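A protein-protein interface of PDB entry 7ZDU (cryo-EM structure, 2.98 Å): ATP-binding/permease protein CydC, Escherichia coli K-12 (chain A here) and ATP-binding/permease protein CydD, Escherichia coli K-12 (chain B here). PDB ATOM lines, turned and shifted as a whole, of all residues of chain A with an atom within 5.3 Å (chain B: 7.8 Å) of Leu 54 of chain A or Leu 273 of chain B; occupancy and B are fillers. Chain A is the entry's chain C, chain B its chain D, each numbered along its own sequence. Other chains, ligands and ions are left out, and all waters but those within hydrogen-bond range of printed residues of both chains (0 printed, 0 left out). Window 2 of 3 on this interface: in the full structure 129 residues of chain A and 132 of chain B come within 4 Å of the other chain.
O of Gly 269 of chain B lies within hydrogen-bond range of OG of Ser 46 of chain A (2.5 Å).
The side-chain hydroxyl of Tyr 59 of chain A lies within hydrogen-bond range of the side-chain carboxylate of Glu 275 of chain B, 3.2 Å away.
The backbone NH (N) of Glu 275 of chain B lies within hydrogen-bond range of the backbone carbonyl oxygen (O) of Phe 270 of chain B, 3.4 Å away.
Gly 269 of chain B touches Phe 42 of chain A.
Tyr 272 of chain B touches Ser 46 of chain A.
Leu 273 of chain B touches Ser 46 of chain A (CG to OG, 3.2 Å).
O of Tyr 272 of chain B touches C of Gly 50 of chain A, at 3.4 Å.
Leu 273 of chain B touches Gly 50 of chain A.
Leu 273 of chain B touches Gly 53 of chain A.
O of Leu 273 of chain B touches CD1 of Leu 54 of chain A, at 3.2 Å.
CD2 of Leu 54 of chain A touches OE2 of Glu 275 of chain B (3.3 Å).
Leu 273 of chain B touches Phe 57 of chain A.
Phe 270 of chain B touches Tyr 59 of chain A (CE1 to CD2, 3.3 Å).
Of chain B, only Leu 273 and Glu 275 come within 4 Å of Leu 54 of chain A.
Of the printed residues of chain A, Leu 273 of chain B touches Ser 46 (3.2 Å), Gly 50 (3.3 Å), Gly 53 (3.8 Å), Leu 54 (3.2 Å), Phe 57 (3.6 Å) and Tyr 59 (3.5 Å).
Gly 53 of chain A touches just one residue of chain B: Leu 273 (3.8 Å).
Printed residues of chain A within 4 Å of Phe 270 of chain B: Tyr 59 (3.3 Å).
Printed residues of chain B within 4 Å of Tyr 59 of chain A: Phe 270 (3.3 Å), Leu 273 (3.5 Å) and Glu 275 (3.2 Å).
Ser 271 of chain B touches none of the printed residues of chain A.
The nearest residue of chain B that does not touch Leu 54 of chain A is Gly 274 of chain B (4.9 Å).
The nearest printed residue of chain B that does not touch Gly 50 of chain A is Gly 274 of chain B (5.5 Å).
Hydrophobic or aromatic side chains of chain B that line the printed part of chain A: Phe 270, Tyr 272 and Leu 273.
Printed residues of chain A that touch a printed residue of chain B: Phe 42, Ser 46, Gly 50, Val 51, Gly 53, Leu 54, Phe 57 and Tyr 59.
Hydrophobic or aromatic side chains of chain A within 4 Å of the printed part of chain B: Phe 42, Leu 54, Phe 57 and Tyr 59.
Among the printed residues, no Asp or Glu carboxylate lies within 4 Å of a Lys or Arg side-chain nitrogen of the other chain.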
ATOM      1  N   PHE A  42     -13.315   6.460  16.059  1.00  0.00           N
ATOM      2  CA  PHE A  42     -13.660   6.984  14.742  1.00  0.00           C
ATOM      3  C   PHE A  42     -14.451   8.281  14.852  1.00  0.00           C
ATOM      4  O   PHE A  42     -14.167   9.250  14.139  1.00  0.00           O
ATOM      5  CB  PHE A  42     -14.440   5.934  13.953  1.00  0.00           C
ATOM      6  CG  PHE A  42     -14.844   6.380  12.577  1.00  0.00           C
ATOM      7  CD1 PHE A  42     -13.994   7.150  11.805  1.00  0.00           C
ATOM      8  CD2 PHE A  42     -16.071   6.020  12.052  1.00  0.00           C
ATOM      9  CE1 PHE A  42     -14.364   7.559  10.543  1.00  0.00           C
ATOM     10  CE2 PHE A  42     -16.445   6.424  10.790  1.00  0.00           C
ATOM     11  CZ  PHE A  42     -15.591   7.194  10.034  1.00  0.00           C
ATOM     12  N   SER A  46     -12.945  11.771  13.706  1.00  0.00           N
ATOM     13  CA  SER A  46     -13.708  12.507  12.704  1.00  0.00           C
ATOM     14  C   SER A  46     -14.076  13.896  13.205  1.00  0.00           C
ATOM     15  O   SER A  46     -14.002  14.875  12.454  1.00  0.00           O
ATOM     16  CB  SER A  46     -14.963  11.723  12.326  1.00  0.00           C
ATOM     17  OG  SER A  46     -15.531  12.216  11.129  1.00  0.00           O
ATOM     18  N   ALA A  49     -11.135  16.211  13.092  1.00  0.00           N
ATOM     19  CA  ALA A  49     -10.833  16.556  11.707  1.00  0.00           C
ATOM     20  C   ALA A  49     -11.779  17.627  11.184  1.00  0.00           C
ATOM     21  O   ALA A  49     -11.347  18.576  10.518  1.00  0.00           O
ATOM     22  CB  ALA A  49     -10.902  15.305  10.832  1.00  0.00           C
ATOM     23  N   GLY A  50     -13.067  17.500  11.476  1.00  0.00           N
ATOM     24  CA  GLY A  50     -14.026  18.487  11.032  1.00  0.00           C
ATOM     25  C   GLY A  50     -14.275  18.419   9.532  1.00  0.00           C
ATOM     26  O   GLY A  50     -13.869  17.491   8.834  1.00  0.00           O
ATOM     27  N   VAL A  51     -14.970  19.448   9.046  1.00  0.00           N
ATOM     28  CA  VAL A  51     -15.276  19.530   7.621  1.00  0.00           C
ATOM     29  C   VAL A  51     -14.008  19.779   6.812  1.00  0.00           C
ATOM     30  O   VAL A  51     -13.847  19.249   5.706  1.00  0.00           O
ATOM     31  CB  VAL A  51     -16.332  20.621   7.370  1.00  0.00           C
ATOM     32  CG1 VAL A  51     -16.675  20.706   5.891  1.00  0.00           C
ATOM     33  CG2 VAL A  51     -17.578  20.354   8.199  1.00  0.00           C
ATOM     34  N   ALA A  52     -13.090  20.587   7.349  1.00  0.00           N
ATOM     35  CA  ALA A  52     -11.892  20.959   6.600  1.00  0.00           C
ATOM     36  C   ALA A  52     -11.022  19.747   6.291  1.00  0.00           C
ATOM     37  O   ALA A  52     -10.516  19.608   5.171  1.00  0.00           O
ATOM     38  CB  ALA A  52     -11.094  22.005   7.379  1.00  0.00           C
ATOM     39  N   GLY A  53     -10.837  18.860   7.264  1.00  0.00           N
ATOM     40  CA  GLY A  53      -9.979  17.707   7.073  1.00  0.00           C
ATOM     41  C   GLY A  53     -10.671  16.534   6.408  1.00  0.00           C
ATOM     42  O   GLY A  53     -10.401  15.377   6.743  1.00  0.00           O
ATOM     43  N   LEU A  54     -11.570  16.823   5.465  1.00  0.00           N
ATOM     44  CA  LEU A  54     -12.297  15.761   4.777  1.00  0.00           C
ATOM     45  C   LEU A  54     -11.350  14.870   3.983  1.00  0.00           C
ATOM     46  O   LEU A  54     -11.366  13.641   4.126  1.00  0.00           O
ATOM     47  CB  LEU A  54     -13.361  16.376   3.863  1.00  0.00           C
ATOM     48  CG  LEU A  54     -14.441  15.505   3.210  1.00  0.00           C
ATOM     49  CD1 LEU A  54     -15.633  16.368   2.833  1.00  0.00           C
ATOM     50  CD2 LEU A  54     -13.924  14.779   1.976  1.00  0.00           C
ATOM     51  N   TYR A  55     -10.516  15.473   3.135  1.00  0.00           N
ATOM     52  CA  TYR A  55      -9.685  14.690   2.228  1.00  0.00           C
ATOM     53  C   TYR A  55      -8.449  14.132   2.923  1.00  0.00           C
ATOM     54  O   TYR A  55      -8.023  13.011   2.626  1.00  0.00           O
ATOM     55  CB  TYR A  55      -9.288  15.541   1.020  1.00  0.00           C
ATOM     56  CG  TYR A  55     -10.451  15.884   0.113  1.00  0.00           C
ATOM     57  CD1 TYR A  55     -11.350  16.887   0.454  1.00  0.00           C
ATOM     58  CD2 TYR A  55     -10.654  15.200  -1.077  1.00  0.00           C
ATOM     59  CE1 TYR A  55     -12.414  17.202  -0.368  1.00  0.00           C
ATOM     60  CE2 TYR A  55     -11.717  15.510  -1.907  1.00  0.00           C
ATOM     61  CZ  TYR A  55     -12.594  16.510  -1.547  1.00  0.00           C
ATOM     62  OH  TYR A  55     -13.653  16.821  -2.367  1.00  0.00           O
ATOM     63  N   SER A  56      -7.857  14.897   3.842  1.00  0.00           N
ATOM     64  CA  SER A  56      -6.648  14.437   4.518  1.00  0.00           C
ATOM     65  C   SER A  56      -6.928  13.227   5.401  1.00  0.00           C
ATOM     66  O   SER A  56      -6.143  12.272   5.424  1.00  0.00           O
ATOM     67  CB  SER A  56      -6.041  15.571   5.341  1.00  0.00           C
ATOM     68  OG  SER A  56      -4.736  15.237   5.780  1.00  0.00           O
ATOM     69  N   PHE A  57      -8.039  13.247   6.133  1.00  0.00           N
ATOM     70  CA  PHE A  57      -8.384  12.147   7.022  1.00  0.00           C
ATOM     71  C   PHE A  57      -8.946  10.983   6.215  1.00  0.00           C
ATOM     72  O   PHE A  57      -9.908  11.147   5.459  1.00  0.00           O
ATOM     73  CB  PHE A  57      -9.396  12.616   8.069  1.00  0.00           C
ATOM     74  CG  PHE A  57      -9.916  11.519   8.953  1.00  0.00           C
ATOM     75  CD1 PHE A  57      -9.101  10.931   9.904  1.00  0.00           C
ATOM     76  CD2 PHE A  57     -11.224  11.084   8.840  1.00  0.00           C
ATOM     77  CE1 PHE A  57      -9.581   9.924  10.720  1.00  0.00           C
ATOM     78  CE2 PHE A  57     -11.709  10.080   9.653  1.00  0.00           C
ATOM     79  CZ  PHE A  57     -10.887   9.499  10.594  1.00  0.00           C
ATOM     80  N   TYR A  59     -11.140   8.090   5.754  1.00  0.00           N
ATOM     81  CA  TYR A  59     -12.403   7.711   6.372  1.00  0.00           C
ATOM     82  C   TYR A  59     -13.030   6.467   5.753  1.00  0.00           C
ATOM     83  O   TYR A  59     -14.168   6.128   6.088  1.00  0.00           O
ATOM     84  CB  TYR A  59     -13.364   8.902   6.323  1.00  0.00           C
ATOM     85  CG  TYR A  59     -13.993   9.176   4.975  1.00  0.00           C
ATOM     86  CD1 TYR A  59     -13.392  10.051   4.079  1.00  0.00           C
ATOM     87  CD2 TYR A  59     -15.202   8.604   4.613  1.00  0.00           C
ATOM     88  CE1 TYR A  59     -13.961  10.319   2.851  1.00  0.00           C
ATOM     89  CE2 TYR A  59     -15.781   8.869   3.387  1.00  0.00           C
ATOM     90  CZ  TYR A  59     -15.156   9.727   2.509  1.00  0.00           C
ATOM     91  OH  TYR A  59     -15.730   9.994   1.288  1.00  0.00           O
ATOM     92  N   TYR B 267     -22.588   6.588  10.302  1.00  0.00           N
ATOM     93  CA  TYR B 267     -23.369   7.792  10.029  1.00  0.00           C
ATOM     94  C   TYR B 267     -22.803   8.998  10.765  1.00  0.00           C
ATOM     95  O   TYR B 267     -22.656  10.080  10.187  1.00  0.00           O
ATOM     96  CB  TYR B 267     -24.831   7.567  10.410  1.00  0.00           C
ATOM     97  CG  TYR B 267     -25.544   8.818  10.857  1.00  0.00           C
ATOM     98  CD1 TYR B 267     -25.999   9.750   9.937  1.00  0.00           C
ATOM     99  CD2 TYR B 267     -25.768   9.065  12.201  1.00  0.00           C
ATOM    100  CE1 TYR B 267     -26.650  10.896  10.345  1.00  0.00           C
ATOM    101  CE2 TYR B 267     -26.417  10.206  12.617  1.00  0.00           C
ATOM    102  CZ  TYR B 267     -26.856  11.116  11.687  1.00  0.00           C
ATOM    103  OH  TYR B 267     -27.504  12.250  12.110  1.00  0.00           O
ATOM    104  N   PHE B 268     -22.481   8.834  12.049  1.00  0.00           N
ATOM    105  CA  PHE B 268     -21.908   9.941  12.805  1.00  0.00           C
ATOM    106  C   PHE B 268     -20.509  10.279  12.315  1.00  0.00           C
ATOM    107  O   PHE B 268     -20.168  11.457  12.163  1.00  0.00           O
ATOM    108  CB  PHE B 268     -21.888   9.612  14.292  1.00  0.00           C
ATOM    109  CG  PHE B 268     -23.139   9.999  15.007  1.00  0.00           C
ATOM    110  CD1 PHE B 268     -24.065   9.044  15.378  1.00  0.00           C
ATOM    111  CD2 PHE B 268     -23.393  11.325  15.304  1.00  0.00           C
ATOM    112  CE1 PHE B 268     -25.215   9.403  16.035  1.00  0.00           C
ATOM    113  CE2 PHE B 268     -24.542  11.687  15.962  1.00  0.00           C
ATOM    114  CZ  PHE B 268     -25.455  10.725  16.328  1.00  0.00           C
ATOM    115  N   GLY B 269     -19.687   9.262  12.060  1.00  0.00           N
ATOM    116  CA  GLY B 269     -18.347   9.516  11.563  1.00  0.00           C
ATOM    117  C   GLY B 269     -18.351  10.260  10.244  1.00  0.00           C
ATOM    118  O   GLY B 269     -17.486  11.101   9.992  1.00  0.00           O
ATOM    119  N   PHE B 270     -19.324   9.961   9.383  1.00  0.00           N
ATOM    120  CA  PHE B 270     -19.423  10.670   8.114  1.00  0.00           C
ATOM    121  C   PHE B 270     -19.983  12.073   8.306  1.00  0.00           C
ATOM    122  O   PHE B 270     -19.544  13.016   7.640  1.00  0.00           O
ATOM    123  CB  PHE B 270     -20.299   9.893   7.134  1.00  0.00           C
ATOM    124  CG  PHE B 270     -19.632   8.687   6.544  1.00  0.00           C
ATOM    125  CD1 PHE B 270     -18.307   8.403   6.818  1.00  0.00           C
ATOM    126  CD2 PHE B 270     -20.328   7.849   5.691  1.00  0.00           C
ATOM    127  CE1 PHE B 270     -17.700   7.291   6.279  1.00  0.00           C
ATOM    128  CE2 PHE B 270     -19.720   6.742   5.139  1.00  0.00           C
ATOM    129  CZ  PHE B 270     -18.404   6.462   5.433  1.00  0.00           C
ATOM    130  N   SER B 271     -20.955  12.225   9.211  1.00  0.00           N
ATOM    131  CA  SER B 271     -21.602  13.519   9.401  1.00  0.00           C
ATOM    132  C   SER B 271     -20.610  14.575   9.868  1.00  0.00           C
ATOM    133  O   SER B 271     -20.647  15.720   9.404  1.00  0.00           O
ATOM    134  CB  SER B 271     -22.754  13.387  10.396  1.00  0.00           C
ATOM    135  OG  SER B 271     -23.616  14.508  10.327  1.00  0.00           O
ATOM    136  N   TYR B 272     -19.715  14.211  10.789  1.00  0.00           N
ATOM    137  CA  TYR B 272     -18.691  15.145  11.239  1.00  0.00           C
ATOM    138  C   TYR B 272     -17.766  15.568  10.108  1.00  0.00           C
ATOM    139  O   TYR B 272     -17.129  16.622  10.203  1.00  0.00           O
ATOM    140  CB  TYR B 272     -17.865  14.526  12.369  1.00  0.00           C
ATOM    141  CG  TYR B 272     -18.637  14.268  13.641  1.00  0.00           C
ATOM    142  CD1 TYR B 272     -19.352  15.278  14.262  1.00  0.00           C
ATOM    143  CD2 TYR B 272     -18.643  13.013  14.225  1.00  0.00           C
ATOM    144  CE1 TYR B 272     -20.053  15.042  15.426  1.00  0.00           C
ATOM    145  CE2 TYR B 272     -19.343  12.768  15.385  1.00  0.00           C
ATOM    146  CZ  TYR B 272     -20.046  13.783  15.981  1.00  0.00           C
ATOM    147  OH  TYR B 272     -20.744  13.539  17.139  1.00  0.00           O
ATOM    148  N   LEU B 273     -17.677  14.773   9.045  1.00  0.00           N
ATOM    149  CA  LEU B 273     -16.790  15.061   7.927  1.00  0.00           C
ATOM    150  C   LEU B 273     -17.482  15.794   6.786  1.00  0.00           C
ATOM    151  O   LEU B 273     -16.815  16.166   5.817  1.00  0.00           O
ATOM    152  CB  LEU B 273     -16.174  13.761   7.407  1.00  0.00           C
ATOM    153  CG  LEU B 273     -14.924  13.314   8.160  1.00  0.00           C
ATOM    154  CD1 LEU B 273     -14.465  11.966   7.659  1.00  0.00           C
ATOM    155  CD2 LEU B 273     -13.817  14.343   8.022  1.00  0.00           C
ATOM    156  N   GLY B 274     -18.790  16.021   6.879  1.00  0.00           N
ATOM    157  CA  GLY B 274     -19.511  16.768   5.871  1.00  0.00           C
ATOM    158  C   GLY B 274     -20.141  15.951   4.765  1.00  0.00           C
ATOM    159  O   GLY B 274     -20.859  16.521   3.934  1.00  0.00           O
ATOM    160  N   GLU B 275     -19.906  14.640   4.719  1.00  0.00           N
ATOM    161  CA  GLU B 275     -20.541  13.804   3.708  1.00  0.00           C
ATOM    162  C   GLU B 275     -22.025  13.581   3.962  1.00  0.00           C
ATOM    163  O   GLU B 275     -22.715  13.073   3.074  1.00  0.00           O
ATOM    164  CB  GLU B 275     -19.832  12.450   3.614  1.00  0.00           C
ATOM    165  CG  GLU B 275     -18.621  12.423   2.690  1.00  0.00           C
ATOM    166  CD  GLU B 275     -17.383  13.067   3.287  1.00  0.00           C
ATOM    167  OE1 GLU B 275     -17.514  13.938   4.173  1.00  0.00           O
ATOM    168  OE2 GLU B 275     -16.269  12.697   2.864  1.00  0.00           O
ATOM    169  N   LEU B 276     -22.530  13.945   5.137  1.00  0.00           N
ATOM    170  CA  LEU B 276     -23.939  13.783   5.461  1.00  0.00           C
ATOM    171  C   LEU B 276     -24.413  15.009   6.228  1.00  0.00           C
ATOM    172  O   LEU B 276     -23.667  15.568   7.036  1.00  0.00           O
ATOM    173  CB  LEU B 276     -24.178  12.509   6.280  1.00  0.00           C
ATOM    174  CG  LEU B 276     -24.124  11.202   5.487  1.00  0.00           C
ATOM    175  CD1 LEU B 276     -24.424  10.011   6.377  1.00  0.00           C
ATOM    176  CD2 LEU B 276     -25.088  11.250   4.316  1.00  0.00           C
ATOM    177  N   VAL B 285     -23.369  19.253  14.063  1.00  0.00           N
ATOM    178  CA  VAL B 285     -23.431  18.045  14.873  1.00  0.00           C
ATOM    179  C   VAL B 285     -22.373  18.116  15.966  1.00  0.00           C
ATOM    180  O   VAL B 285     -21.209  18.456  15.712  1.00  0.00           O
ATOM    181  CB  VAL B 285     -23.238  16.796  13.997  1.00  0.00           C
ATOM    182  CG1 VAL B 285     -23.417  15.535  14.824  1.00  0.00           C
ATOM    183  CG2 VAL B 285     -24.195  16.814  12.823  1.00  0.00           C
